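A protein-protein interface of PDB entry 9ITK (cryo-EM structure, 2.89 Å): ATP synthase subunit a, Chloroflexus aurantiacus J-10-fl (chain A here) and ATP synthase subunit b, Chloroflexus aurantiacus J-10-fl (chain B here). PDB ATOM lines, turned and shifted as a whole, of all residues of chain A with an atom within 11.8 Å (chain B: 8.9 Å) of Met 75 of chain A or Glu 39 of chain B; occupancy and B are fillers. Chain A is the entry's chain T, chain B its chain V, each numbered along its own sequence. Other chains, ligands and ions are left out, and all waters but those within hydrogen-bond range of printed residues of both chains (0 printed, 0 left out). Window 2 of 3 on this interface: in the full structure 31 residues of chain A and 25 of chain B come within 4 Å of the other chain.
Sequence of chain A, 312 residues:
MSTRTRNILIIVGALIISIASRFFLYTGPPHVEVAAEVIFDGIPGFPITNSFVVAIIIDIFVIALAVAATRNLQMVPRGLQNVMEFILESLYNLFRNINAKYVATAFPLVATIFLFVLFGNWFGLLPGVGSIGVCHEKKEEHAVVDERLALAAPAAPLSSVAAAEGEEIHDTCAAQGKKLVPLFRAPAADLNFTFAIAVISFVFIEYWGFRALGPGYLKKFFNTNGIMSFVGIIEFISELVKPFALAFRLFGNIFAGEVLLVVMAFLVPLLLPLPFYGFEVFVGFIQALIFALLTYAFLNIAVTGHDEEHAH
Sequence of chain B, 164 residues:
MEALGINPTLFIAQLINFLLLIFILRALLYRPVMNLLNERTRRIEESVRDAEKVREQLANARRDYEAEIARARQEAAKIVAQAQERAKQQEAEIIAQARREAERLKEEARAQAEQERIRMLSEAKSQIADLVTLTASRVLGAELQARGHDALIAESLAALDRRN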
ATOM      1  N   ALA A  69      13.847  26.587   1.306  1.00  0.00           N
ATOM      2  CA  ALA A  69      14.800  26.569   2.409  1.00  0.00           C
ATOM      3  C   ALA A  69      15.919  25.566   2.156  1.00  0.00           C
ATOM      4  O   ALA A  69      17.082  25.829   2.482  1.00  0.00           O
ATOM      5  CB  ALA A  69      14.081  26.252   3.720  1.00  0.00           C
ATOM      6  N   THR A  70      15.586  24.408   1.582  1.00  0.00           N
ATOM      7  CA  THR A  70      16.607  23.407   1.292  1.00  0.00           C
ATOM      8  C   THR A  70      17.495  23.832   0.126  1.00  0.00           C
ATOM      9  O   THR A  70      18.648  23.394   0.035  1.00  0.00           O
ATOM     10  CB  THR A  70      15.947  22.058   0.999  1.00  0.00           C
ATOM     11  OG1 THR A  70      14.989  21.764   2.023  1.00  0.00           O
ATOM     12  CG2 THR A  70      16.983  20.943   0.968  1.00  0.00           C
ATOM     13  N   ARG A  71      16.983  24.686  -0.764  1.00  0.00           N
ATOM     14  CA  ARG A  71      17.770  25.124  -1.913  1.00  0.00           C
ATOM     15  C   ARG A  71      19.003  25.905  -1.475  1.00  0.00           C
ATOM     16  O   ARG A  71      20.090  25.733  -2.039  1.00  0.00           O
ATOM     17  CB  ARG A  71      16.906  25.968  -2.849  1.00  0.00           C
ATOM     18  CG  ARG A  71      17.396  26.000  -4.287  1.00  0.00           C
ATOM     19  CD  ARG A  71      16.892  27.234  -5.018  1.00  0.00           C
ATOM     20  NE  ARG A  71      15.450  27.202  -5.232  1.00  0.00           N
ATOM     21  CZ  ARG A  71      14.843  26.471  -6.158  1.00  0.00           C
ATOM     22  NH1 ARG A  71      15.525  25.691  -6.980  1.00  0.00           N
ATOM     23  NH2 ARG A  71      13.519  26.527  -6.263  1.00  0.00           N
ATOM     24  N   ASN A  72      18.856  26.767  -0.474  1.00  0.00           N
ATOM     25  CA  ASN A  72      19.957  27.564   0.049  1.00  0.00           C
ATOM     26  C   ASN A  72      20.498  26.898   1.309  1.00  0.00           C
ATOM     27  O   ASN A  72      19.766  26.728   2.290  1.00  0.00           O
ATOM     28  CB  ASN A  72      19.504  28.993   0.346  1.00  0.00           C
ATOM     29  CG  ASN A  72      19.412  29.848  -0.904  1.00  0.00           C
ATOM     30  OD1 ASN A  72      20.282  29.794  -1.772  1.00  0.00           O
ATOM     31  ND2 ASN A  72      18.353  30.644  -0.999  1.00  0.00           N
ATOM     32  N   LEU A  73      21.778  26.527   1.281  1.00  0.00           N
ATOM     33  CA  LEU A  73      22.424  25.836   2.389  1.00  0.00           C
ATOM     34  C   LEU A  73      23.528  26.678   3.019  1.00  0.00           C
ATOM     35  O   LEU A  73      24.499  26.139   3.554  1.00  0.00           O
ATOM     36  CB  LEU A  73      22.981  24.490   1.926  1.00  0.00           C
ATOM     37  CG  LEU A  73      21.977  23.480   1.366  1.00  0.00           C
ATOM     38  CD1 LEU A  73      21.938  23.540  -0.155  1.00  0.00           C
ATOM     39  CD2 LEU A  73      22.308  22.075   1.841  1.00  0.00           C
ATOM     40  N   GLN A  74      23.393  28.000   2.958  1.00  0.00           N
ATOM     41  CA  GLN A  74      24.416  28.886   3.496  1.00  0.00           C
ATOM     42  C   GLN A  74      24.512  28.745   5.010  1.00  0.00           C
ATOM     43  O   GLN A  74      23.505  28.575   5.701  1.00  0.00           O
ATOM     44  CB  GLN A  74      24.111  30.336   3.127  1.00  0.00           C
ATOM     45  CG  GLN A  74      24.365  30.675   1.668  1.00  0.00           C
ATOM     46  CD  GLN A  74      23.210  30.274   0.772  1.00  0.00           C
ATOM     47  OE1 GLN A  74      22.108  30.805   0.888  1.00  0.00           O
ATOM     48  NE2 GLN A  74      23.459  29.329  -0.127  1.00  0.00           N
ATOM     49  N   MET A  75      25.741  28.816   5.527  1.00  0.00           N
ATOM     50  CA  MET A  75      25.942  28.779   6.970  1.00  0.00           C
ATOM     51  C   MET A  75      25.391  30.018   7.660  1.00  0.00           C
ATOM     52  O   MET A  75      25.173  29.989   8.875  1.00  0.00           O
ATOM     53  CB  MET A  75      27.426  28.616   7.297  1.00  0.00           C
ATOM     54  CG  MET A  75      28.025  27.291   6.852  1.00  0.00           C
ATOM     55  SD  MET A  75      27.258  25.865   7.643  1.00  0.00           S
ATOM     56  CE  MET A  75      26.193  25.269   6.332  1.00  0.00           C
ATOM     57  N   VAL A  76      25.162  31.098   6.920  1.00  0.00           N
ATOM     58  CA  VAL A  76      24.530  32.290   7.477  1.00  0.00           C
ATOM     59  C   VAL A  76      23.115  32.393   6.914  1.00  0.00           C
ATOM     60  O   VAL A  76      22.924  32.782   5.753  1.00  0.00           O
ATOM     61  CB  VAL A  76      25.372  33.548   7.206  1.00  0.00           C
ATOM     62  CG1 VAL A  76      26.634  33.508   8.045  1.00  0.00           C
ATOM     63  CG2 VAL A  76      25.759  33.646   5.736  1.00  0.00           C
ATOM     64  N   PRO A  77      22.099  32.029   7.691  1.00  0.00           N
ATOM     65  CA  PRO A  77      20.728  32.056   7.174  1.00  0.00           C
ATOM     66  C   PRO A  77      20.248  33.471   6.898  1.00  0.00           C
ATOM     67  O   PRO A  77      20.615  34.427   7.587  1.00  0.00           O
ATOM     68  CB  PRO A  77      19.913  31.401   8.294  1.00  0.00           C
ATOM     69  CG  PRO A  77      20.740  31.582   9.522  1.00  0.00           C
ATOM     70  CD  PRO A  77      22.164  31.513   9.067  1.00  0.00           C
ATOM     71  N   ARG A  78      19.406  33.590   5.874  1.00  0.00           N
ATOM     72  CA  ARG A  78      18.801  34.857   5.489  1.00  0.00           C
ATOM     73  C   ARG A  78      17.643  34.570   4.546  1.00  0.00           C
ATOM     74  O   ARG A  78      17.749  33.697   3.681  1.00  0.00           O
ATOM     75  CB  ARG A  78      19.822  35.785   4.815  1.00  0.00           C
ATOM     76  CG  ARG A  78      19.266  37.151   4.437  1.00  0.00           C
ATOM     77  CD  ARG A  78      18.550  37.800   5.612  1.00  0.00           C
ATOM     78  NE  ARG A  78      17.836  39.008   5.219  1.00  0.00           N
ATOM     79  CZ  ARG A  78      18.394  40.206   5.107  1.00  0.00           C
ATOM     80  NH1 ARG A  78      19.679  40.397   5.356  1.00  0.00           N
ATOM     81  NH2 ARG A  78      17.642  41.240   4.737  1.00  0.00           N
ATOM     82  N   GLY A  79      16.547  35.302   4.721  1.00  0.00           N
ATOM     83  CA  GLY A  79      15.386  35.127   3.871  1.00  0.00           C
ATOM     84  C   GLY A  79      14.466  34.017   4.332  1.00  0.00           C
ATOM     85  O   GLY A  79      14.419  33.696   5.523  1.00  0.00           O
ATOM     86  N   GLN A  81      14.750  30.936   4.016  1.00  0.00           N
ATOM     87  CA  GLN A  81      15.472  29.819   4.614  1.00  0.00           C
ATOM     88  C   GLN A  81      15.801  30.091   6.077  1.00  0.00           C
ATOM     89  O   GLN A  81      15.871  29.155   6.881  1.00  0.00           O
ATOM     90  CB  GLN A  81      16.735  29.528   3.799  1.00  0.00           C
ATOM     91  CG  GLN A  81      17.793  28.688   4.499  1.00  0.00           C
ATOM     92  CD  GLN A  81      18.843  29.534   5.187  1.00  0.00           C
ATOM     93  OE1 GLN A  81      18.960  30.729   4.920  1.00  0.00           O
ATOM     94  NE2 GLN A  81      19.616  28.918   6.072  1.00  0.00           N
ATOM     95  N   ASN A  82      15.989  31.361   6.443  1.00  0.00           N
ATOM     96  CA  ASN A  82      16.263  31.699   7.836  1.00  0.00           C
ATOM     97  C   ASN A  82      15.042  31.468   8.717  1.00  0.00           C
ATOM     98  O   ASN A  82      15.151  30.897   9.808  1.00  0.00           O
ATOM     99  CB  ASN A  82      16.725  33.152   7.943  1.00  0.00           C
ATOM    100  CG  ASN A  82      17.083  33.545   9.363  1.00  0.00           C
ATOM    101  OD1 ASN A  82      17.388  32.693  10.199  1.00  0.00           O
ATOM    102  ND2 ASN A  82      17.041  34.842   9.646  1.00  0.00           N
ATOM    103  N   VAL A  83      13.867  31.911   8.261  1.00  0.00           N
ATOM    104  CA  VAL A  83      12.674  31.835   9.099  1.00  0.00           C
ATOM    105  C   VAL A  83      12.278  30.384   9.340  1.00  0.00           C
ATOM    106  O   VAL A  83      11.821  30.028  10.433  1.00  0.00           O
ATOM    107  CB  VAL A  83      11.526  32.655   8.483  1.00  0.00           C
ATOM    108  CG1 VAL A  83      11.937  34.108   8.338  1.00  0.00           C
ATOM    109  CG2 VAL A  83      11.112  32.091   7.135  1.00  0.00           C
ATOM    110  N   GLU A  85      14.446  27.934   9.360  1.00  0.00           N
ATOM    111  CA  GLU A  85      15.436  27.471  10.323  1.00  0.00           C
ATOM    112  C   GLU A  85      15.004  27.812  11.742  1.00  0.00           C
ATOM    113  O   GLU A  85      15.110  26.979  12.648  1.00  0.00           O
ATOM    114  CB  GLU A  85      16.804  28.084  10.013  1.00  0.00           C
ATOM    115  CG  GLU A  85      17.987  27.676  10.928  1.00  0.00           C
ATOM    116  CD  GLU A  85      18.122  26.179  11.230  1.00  0.00           C
ATOM    117  OE1 GLU A  85      19.068  25.823  11.963  1.00  0.00           O
ATOM    118  OE2 GLU A  85      17.347  25.346  10.719  1.00  0.00           O
ATOM    119  N   PHE A  86      14.494  29.029  11.946  1.00  0.00           N
ATOM    120  CA  PHE A  86      14.066  29.452  13.275  1.00  0.00           C
ATOM    121  C   PHE A  86      12.863  28.651  13.756  1.00  0.00           C
ATOM    122  O   PHE A  86      12.786  28.280  14.933  1.00  0.00           O
ATOM    123  CB  PHE A  86      13.747  30.947  13.264  1.00  0.00           C
ATOM    124  CG  PHE A  86      13.084  31.439  14.517  1.00  0.00           C
ATOM    125  CD1 PHE A  86      13.690  31.271  15.751  1.00  0.00           C
ATOM    126  CD2 PHE A  86      11.859  32.077  14.460  1.00  0.00           C
ATOM    127  CE1 PHE A  86      13.082  31.727  16.905  1.00  0.00           C
ATOM    128  CE2 PHE A  86      11.245  32.536  15.610  1.00  0.00           C
ATOM    129  CZ  PHE A  86      11.858  32.360  16.835  1.00  0.00           C
ATOM    130  N   GLU A  89      13.870  24.891  14.831  1.00  0.00           N
ATOM    131  CA  GLU A  89      14.622  24.773  16.079  1.00  0.00           C
ATOM    132  C   GLU A  89      13.764  25.156  17.277  1.00  0.00           C
ATOM    133  O   GLU A  89      13.906  24.574  18.358  1.00  0.00           O
ATOM    134  CB  GLU A  89      15.884  25.635  16.033  1.00  0.00           C
ATOM    135  CG  GLU A  89      15.650  27.084  15.656  1.00  0.00           C
ATOM    136  CD  GLU A  89      16.898  27.931  15.800  1.00  0.00           C
ATOM    137  OE1 GLU A  89      17.976  27.360  16.072  1.00  0.00           O
ATOM    138  OE2 GLU A  89      16.803  29.166  15.641  1.00  0.00           O
ATOM    139  N   TYR A  92      11.884  22.277  17.939  1.00  0.00           N
ATOM    140  CA  TYR A  92      12.840  21.280  18.406  1.00  0.00           C
ATOM    141  C   TYR A  92      13.235  21.542  19.854  1.00  0.00           C
ATOM    142  O   TYR A  92      13.409  20.602  20.638  1.00  0.00           O
ATOM    143  CB  TYR A  92      14.070  21.276  17.500  1.00  0.00           C
ATOM    144  CG  TYR A  92      15.109  20.244  17.868  1.00  0.00           C
ATOM    145  CD1 TYR A  92      14.917  18.903  17.570  1.00  0.00           C
ATOM    146  CD2 TYR A  92      16.285  20.610  18.509  1.00  0.00           C
ATOM    147  CE1 TYR A  92      15.863  17.954  17.900  1.00  0.00           C
ATOM    148  CE2 TYR A  92      17.237  19.668  18.844  1.00  0.00           C
ATOM    149  CZ  TYR A  92      17.021  18.342  18.538  1.00  0.00           C
ATOM    150  OH  TYR A  92      17.966  17.399  18.870  1.00  0.00           O
ATOM    151  N   ARG B  31      15.661  16.035   7.875  1.00  0.00           N
ATOM    152  CA  ARG B  31      17.030  15.530   7.957  1.00  0.00           C
ATOM    153  C   ARG B  31      18.061  16.572   7.540  1.00  0.00           C
ATOM    154  O   ARG B  31      19.071  16.718   8.251  1.00  0.00           O
ATOM    155  CB  ARG B  31      17.154  14.236   7.143  1.00  0.00           C
ATOM    156  CG  ARG B  31      16.148  13.169   7.546  1.00  0.00           C
ATOM    157  CD  ARG B  31      16.467  11.817   6.930  1.00  0.00           C
ATOM    158  NE  ARG B  31      17.233  10.974   7.840  1.00  0.00           N
ATOM    159  CZ  ARG B  31      17.402   9.667   7.687  1.00  0.00           C
ATOM    160  NH1 ARG B  31      16.872   9.016   6.665  1.00  0.00           N
ATOM    161  NH2 ARG B  31      18.118   8.996   8.585  1.00  0.00           N
ATOM    162  N   PRO B  32      17.901  17.308   6.431  1.00  0.00           N
ATOM    163  CA  PRO B  32      18.870  18.381   6.144  1.00  0.00           C
ATOM    164  C   PRO B  32      18.966  19.432   7.237  1.00  0.00           C
ATOM    165  O   PRO B  32      20.071  19.896   7.544  1.00  0.00           O
ATOM    166  CB  PRO B  32      18.345  18.975   4.829  1.00  0.00           C
ATOM    167  CG  PRO B  32      17.630  17.853   4.183  1.00  0.00           C
ATOM    168  CD  PRO B  32      16.974  17.105   5.302  1.00  0.00           C
ATOM    169  N   VAL B  33      17.840  19.821   7.839  1.00  0.00           N
ATOM    170  CA  VAL B  33      17.886  20.796   8.925  1.00  0.00           C
ATOM    171  C   VAL B  33      18.511  20.183  10.171  1.00  0.00           C
ATOM    172  O   VAL B  33      19.297  20.833  10.871  1.00  0.00           O
ATOM    173  CB  VAL B  33      16.480  21.357   9.207  1.00  0.00           C
ATOM    174  CG1 VAL B  33      16.518  22.294  10.397  1.00  0.00           C
ATOM    175  CG2 VAL B  33      15.961  22.100   7.988  1.00  0.00           C
ATOM    176  N   MET B  34      18.172  18.927  10.473  1.00  0.00           N
ATOM    177  CA  MET B  34      18.799  18.253  11.604  1.00  0.00           C
ATOM    178  C   MET B  34      20.301  18.115  11.394  1.00  0.00           C
ATOM    179  O   MET B  34      21.089  18.328  12.322  1.00  0.00           O
ATOM    180  CB  MET B  34      18.159  16.881  11.821  1.00  0.00           C
ATOM    181  CG  MET B  34      18.883  16.019  12.842  1.00  0.00           C
ATOM    182  SD  MET B  34      18.243  14.338  12.934  1.00  0.00           S
ATOM    183  CE  MET B  34      18.555  13.954  14.655  1.00  0.00           C
ATOM    184  N   ASN B  35      20.716  17.768  10.173  1.00  0.00           N
ATOM    185  CA  ASN B  35      22.139  17.661   9.876  1.00  0.00           C
ATOM    186  C   ASN B  35      22.836  19.007  10.018  1.00  0.00           C
ATOM    187  O   ASN B  35      23.959  19.082  10.527  1.00  0.00           O
ATOM    188  CB  ASN B  35      22.339  17.093   8.471  1.00  0.00           C
ATOM    189  CG  ASN B  35      21.915  15.641   8.367  1.00  0.00           C
ATOM    190  OD1 ASN B  35      22.039  14.877   9.325  1.00  0.00           O
ATOM    191  ND2 ASN B  35      21.412  15.253   7.202  1.00  0.00           N
ATOM    192  N   LEU B  36      22.186  20.085   9.569  1.00  0.00           N
ATOM    193  CA  LEU B  36      22.754  21.417   9.750  1.00  0.00           C
ATOM    194  C   LEU B  36      22.885  21.763  11.228  1.00  0.00           C
ATOM    195  O   LEU B  36      23.880  22.363  11.648  1.00  0.00           O
ATOM    196  CB  LEU B  36      21.898  22.460   9.035  1.00  0.00           C
ATOM    197  CG  LEU B  36      22.067  22.574   7.521  1.00  0.00           C
ATOM    198  CD1 LEU B  36      21.125  23.625   6.957  1.00  0.00           C
ATOM    199  CD2 LEU B  36      23.507  22.896   7.170  1.00  0.00           C
ATOM    200  N   LEU B  37      21.881  21.402  12.030  1.00  0.00           N
ATOM    201  CA  LEU B  37      21.952  21.665  13.462  1.00  0.00           C
ATOM    202  C   LEU B  37      23.067  20.859  14.117  1.00  0.00           C
ATOM    203  O   LEU B  37      23.789  21.375  14.977  1.00  0.00           O
ATOM    204  CB  LEU B  37      20.596  21.370  14.112  1.00  0.00           C
ATOM    205  CG  LEU B  37      20.418  21.368  15.635  1.00  0.00           C
ATOM    206  CD1 LEU B  37      18.981  21.717  15.975  1.00  0.00           C
ATOM    207  CD2 LEU B  37      20.768  20.018  16.250  1.00  0.00           C
ATOM    208  N   ASN B  38      23.218  19.589  13.729  1.00  0.00           N
ATOM    209  CA  ASN B  38      24.260  18.758  14.325  1.00  0.00           C
ATOM    210  C   ASN B  38      25.653  19.271  13.977  1.00  0.00           C
ATOM    211  O   ASN B  38      26.532  19.327  14.845  1.00  0.00           O
ATOM    212  CB  ASN B  38      24.102  17.305  13.879  1.00  0.00           C
ATOM    213  CG  ASN B  38      22.929  16.615  14.545  1.00  0.00           C
ATOM    214  OD1 ASN B  38      21.988  16.186  13.881  1.00  0.00           O
ATOM    215  ND2 ASN B  38      22.984  16.504  15.867  1.00  0.00           N
ATOM    216  N   GLU B  39      25.877  19.646  12.716  1.00  0.00           N
ATOM    217  CA  GLU B  39      27.204  20.107  12.322  1.00  0.00           C
ATOM    218  C   GLU B  39      27.531  21.455  12.956  1.00  0.00           C
ATOM    219  O   GLU B  39      28.677  21.697  13.348  1.00  0.00           O
ATOM    220  CB  GLU B  39      27.319  20.172  10.797  1.00  0.00           C
ATOM    221  CG  GLU B  39      26.428  21.199  10.119  1.00  0.00           C
ATOM    222  CD  GLU B  39      27.111  22.543   9.950  1.00  0.00           C
ATOM    223  OE1 GLU B  39      28.358  22.581   9.962  1.00  0.00           O
ATOM    224  OE2 GLU B  39      26.401  23.559   9.806  1.00  0.00           O
ATOM    225  N   ARG B  40      26.537  22.340  13.073  1.00  0.00           N
ATOM    226  CA  ARG B  40      26.769  23.627  13.721  1.00  0.00           C
ATOM    227  C   ARG B  40      27.154  23.442  15.181  1.00  0.00           C
ATOM    228  O   ARG B  40      28.076  24.098  15.677  1.00  0.00           O
ATOM    229  CB  ARG B  40      25.523  24.502  13.606  1.00  0.00           C
ATOM    230  CG  ARG B  40      25.497  25.397  12.383  1.00  0.00           C
ATOM    231  CD  ARG B  40      24.248  26.257  12.381  1.00  0.00           C
ATOM    232  NE  ARG B  40      23.731  26.473  11.035  1.00  0.00           N
ATOM    233  CZ  ARG B  40      22.677  25.847  10.530  1.00  0.00           C
ATOM    234  NH1 ARG B  40      22.003  24.952  11.233  1.00  0.00           N
ATOM    235  NH2 ARG B  40      22.289  26.126   9.288  1.00  0.00           N
ATOM    236  N   THR B  41      26.454  22.551  15.886  1.00  0.00           N
ATOM    237  CA  THR B  41      26.840  22.227  17.255  1.00  0.00           C
ATOM    238  C   THR B  41      28.198  21.541  17.293  1.00  0.00           C
ATOM    239  O   THR B  41      29.011  21.807  18.185  1.00  0.00           O
ATOM    240  CB  THR B  41      25.776  21.346  17.908  1.00  0.00           C
ATOM    241  OG1 THR B  41      24.475  21.839  17.570  1.00  0.00           O
ATOM    242  CG2 THR B  41      25.938  21.355  19.419  1.00  0.00           C
ATOM    243  N   ARG B  42      28.458  20.642  16.341  1.00  0.00           N
ATOM    244  CA  ARG B  42      29.770  20.009  16.270  1.00  0.00           C
ATOM    245  C   ARG B  42      30.854  21.030  15.948  1.00  0.00           C
ATOM    246  O   ARG B  42      31.944  20.993  16.529  1.00  0.00           O
ATOM    247  CB  ARG B  42      29.754  18.890  15.228  1.00  0.00           C
ATOM    248  CG  ARG B  42      31.008  18.027  15.208  1.00  0.00           C
ATOM    249  CD  ARG B  42      31.964  18.457  14.106  1.00  0.00           C
ATOM    250  NE  ARG B  42      31.269  18.701  12.847  1.00  0.00           N
ATOM    251  CZ  ARG B  42      31.565  19.682  12.006  1.00  0.00           C
ATOM    252  NH1 ARG B  42      32.535  20.543  12.262  1.00  0.00           N
ATOM    253  NH2 ARG B  42      30.867  19.803  10.881  1.00  0.00           N
ATOM    254  N   ARG B  43      30.570  21.949  15.023  1.00  0.00           N
ATOM    255  CA  ARG B  43      31.575  22.925  14.614  1.00  0.00           C
ATOM    256  C   ARG B  43      31.900  23.895  15.744  1.00  0.00           C
ATOM    257  O   ARG B  43      33.062  24.280  15.920  1.00  0.00           O
ATOM    258  CB  ARG B  43      31.103  23.664  13.358  1.00  0.00           C
ATOM    259  CG  ARG B  43      32.105  24.648  12.766  1.00  0.00           C
ATOM    260  CD  ARG B  43      31.434  25.938  12.289  1.00  0.00           C
ATOM    261  NE  ARG B  43      30.391  26.446  13.175  1.00  0.00           N
ATOM    262  CZ  ARG B  43      30.577  26.819  14.435  1.00  0.00           C
ATOM    263  NH1 ARG B  43      31.779  26.832  14.985  1.00  0.00           N
ATOM    264  NH2 ARG B  43      29.530  27.217  15.153  1.00  0.00           N
ATOM    265  N   ILE B  44      30.894  24.304  16.522  1.00  0.00           N
ATOM    266  CA  ILE B  44      31.169  25.192  17.648  1.00  0.00           C
ATOM    267  C   ILE B  44      31.944  24.461  18.737  1.00  0.00           C
ATOM    268  O   ILE B  44      32.744  25.075  19.454  1.00  0.00           O
ATOM    269  CB  ILE B  44      29.869  25.822  18.184  1.00  0.00           C
ATOM    270  CG1 ILE B  44      30.191  27.071  19.005  1.00  0.00           C
ATOM    271  CG2 ILE B  44      29.082  24.840  19.029  1.00  0.00           C
ATOM    272  CD1 ILE B  44      30.732  28.213  18.181  1.00  0.00           C
ATOM    273  N   GLU B  45      31.732  23.151  18.888  1.00  0.00           N
ATOM    274  CA  GLU B  45      32.555  22.384  19.817  1.00  0.00           C
ATOM    275  C   GLU B  45      33.944  22.133  19.249  1.00  0.00           C
ATOM    276  O   GLU B  45      34.919  22.059  20.007  1.00  0.00           O
ATOM    277  CB  GLU B  45      31.873  21.064  20.170  1.00  0.00           C
ATOM    278  CG  GLU B  45      30.551  21.231  20.898  1.00  0.00           C
ATOM    279  CD  GLU B  45      30.664  22.126  22.118  1.00  0.00           C
ATOM    280  OE1 GLU B  45      31.651  21.992  22.872  1.00  0.00           O
ATOM    281  OE2 GLU B  45      29.769  22.972  22.316  1.00  0.00           O
ATOM    282  N   GLU B  46      34.055  21.993  17.927  1.00  0.00           N
ATOM    283  CA  GLU B  46      35.369  21.888  17.304  1.00  0.00           C
ATOM    284  C   GLU B  46      36.176  23.160  17.524  1.00  0.00           C
ATOM    285  O   GLU B  46      37.386  23.104  17.772  1.00  0.00           O
ATOM    286  CB  GLU B  46      35.220  21.592  15.812  1.00  0.00           C
ATOM    287  CG  GLU B  46      36.480  21.062  15.154  1.00  0.00           C
ATOM    288  CD  GLU B  46      36.788  19.635  15.555  1.00  0.00           C
ATOM    289  OE1 GLU B  46      35.838  18.883  15.855  1.00  0.00           O
ATOM    290  OE2 GLU B  46      37.982  19.267  15.574  1.00  0.00           O
ATOM    291  N   SER B  47      35.519  24.320  17.438  1.00  0.00           N
ATOM    292  CA  SER B  47      36.197  25.579  17.720  1.00  0.00           C
ATOM    293  C   SER B  47      36.625  25.671  19.179  1.00  0.00           C
ATOM    294  O   SER B  47      37.639  26.307  19.486  1.00  0.00           O
ATOM    295  CB  SER B  47      35.293  26.755  17.354  1.00  0.00           C
ATOM    296  OG  SER B  47      35.818  27.977  17.841  1.00  0.00           O
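The guanidinium group (NH1) of Arg 40 of chain B is in salt-bridge range of the side-chain carboxylate (OE1) of Glu 85 of chain A.
OE2 of Glu 39 of chain B sits close to SD of Met 75 of chain A (3.3 Å).
NH1 of Arg 40 of chain B lies within hydrogen-bond range of O of Leu 36 of chain B.
O of Leu 37 of chain B is in hydrogen-bond range of OG1 of Thr 41 of chain B, at 2.7 Å.
The side-chain carboxylate (OE1) of Glu 39 of chain B is in salt-bridge range of the guanidinium group (NH2) of Arg 42 of chain B (3.9 Å).
The guanidinium group (NH2) of Arg 43 of chain B lies within hydrogen-bond range of the backbone carbonyl oxygen (O) of Arg 40 of chain B, 3.5 Å away.
Among the printed residues, merely in contact across the chains: Met 75 of chain A with Leu 36 of chain B (3.7 Å), Glu 85 of chain A with Val 33 of chain B (3.2 Å) and Tyr 92 of chain A with Leu 37 of chain B (3.9 Å).
Met 75 of chain A touches just these residues of chain B: Leu 36 and Glu 39.
Of the printed residues of chain A, Glu 39 of chain B touches Met 75 (3.3 Å).
No residue of chain B comes within 4 Å of Val 76 of chain A.
Leu 36 of chain B touches just one residue of chain A: Met 75.
Of the printed residues of chain A, Arg 40 of chain B touches Glu 85 (3.1 Å).
No residue of chain A comes within 4 Å of Thr 41 of chain B.
No residue of chain A comes within 4 Å of Arg 42 of chain B.
No residue of chain A comes within 4 Å of Arg 43 of chain B.
Printed residues of chain B within 4 Å of Tyr 92 of chain A: Leu 37 (3.9 Å).
Of the printed residues of chain A, Val 33 of chain B touches Glu 85.
Of the printed residues of chain A, Leu 37 of chain B touches Tyr 92 (3.9 Å).
Asn 35 of chain B touches none of the printed residues of chain A.
Arg 31 of chain B touches none of the printed residues of chain A.
The nearest residue of chain A that does not touch Glu 39 of chain B is Leu 73 of chain A (7.0 Å).
The nearest printed residue of chain B that does not touch Glu 85 of chain A is Leu 37 of chain B (5.2 Å).
Printed residues of chain B that touch a printed residue of chain A: Val 33, Leu 36, Leu 37, Glu 39 and Arg 40.
Of the 18 printed residues of chain A, 3 touch a printed residue of chain B.
Among the printed residues, 5 pairs touch across the chains.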
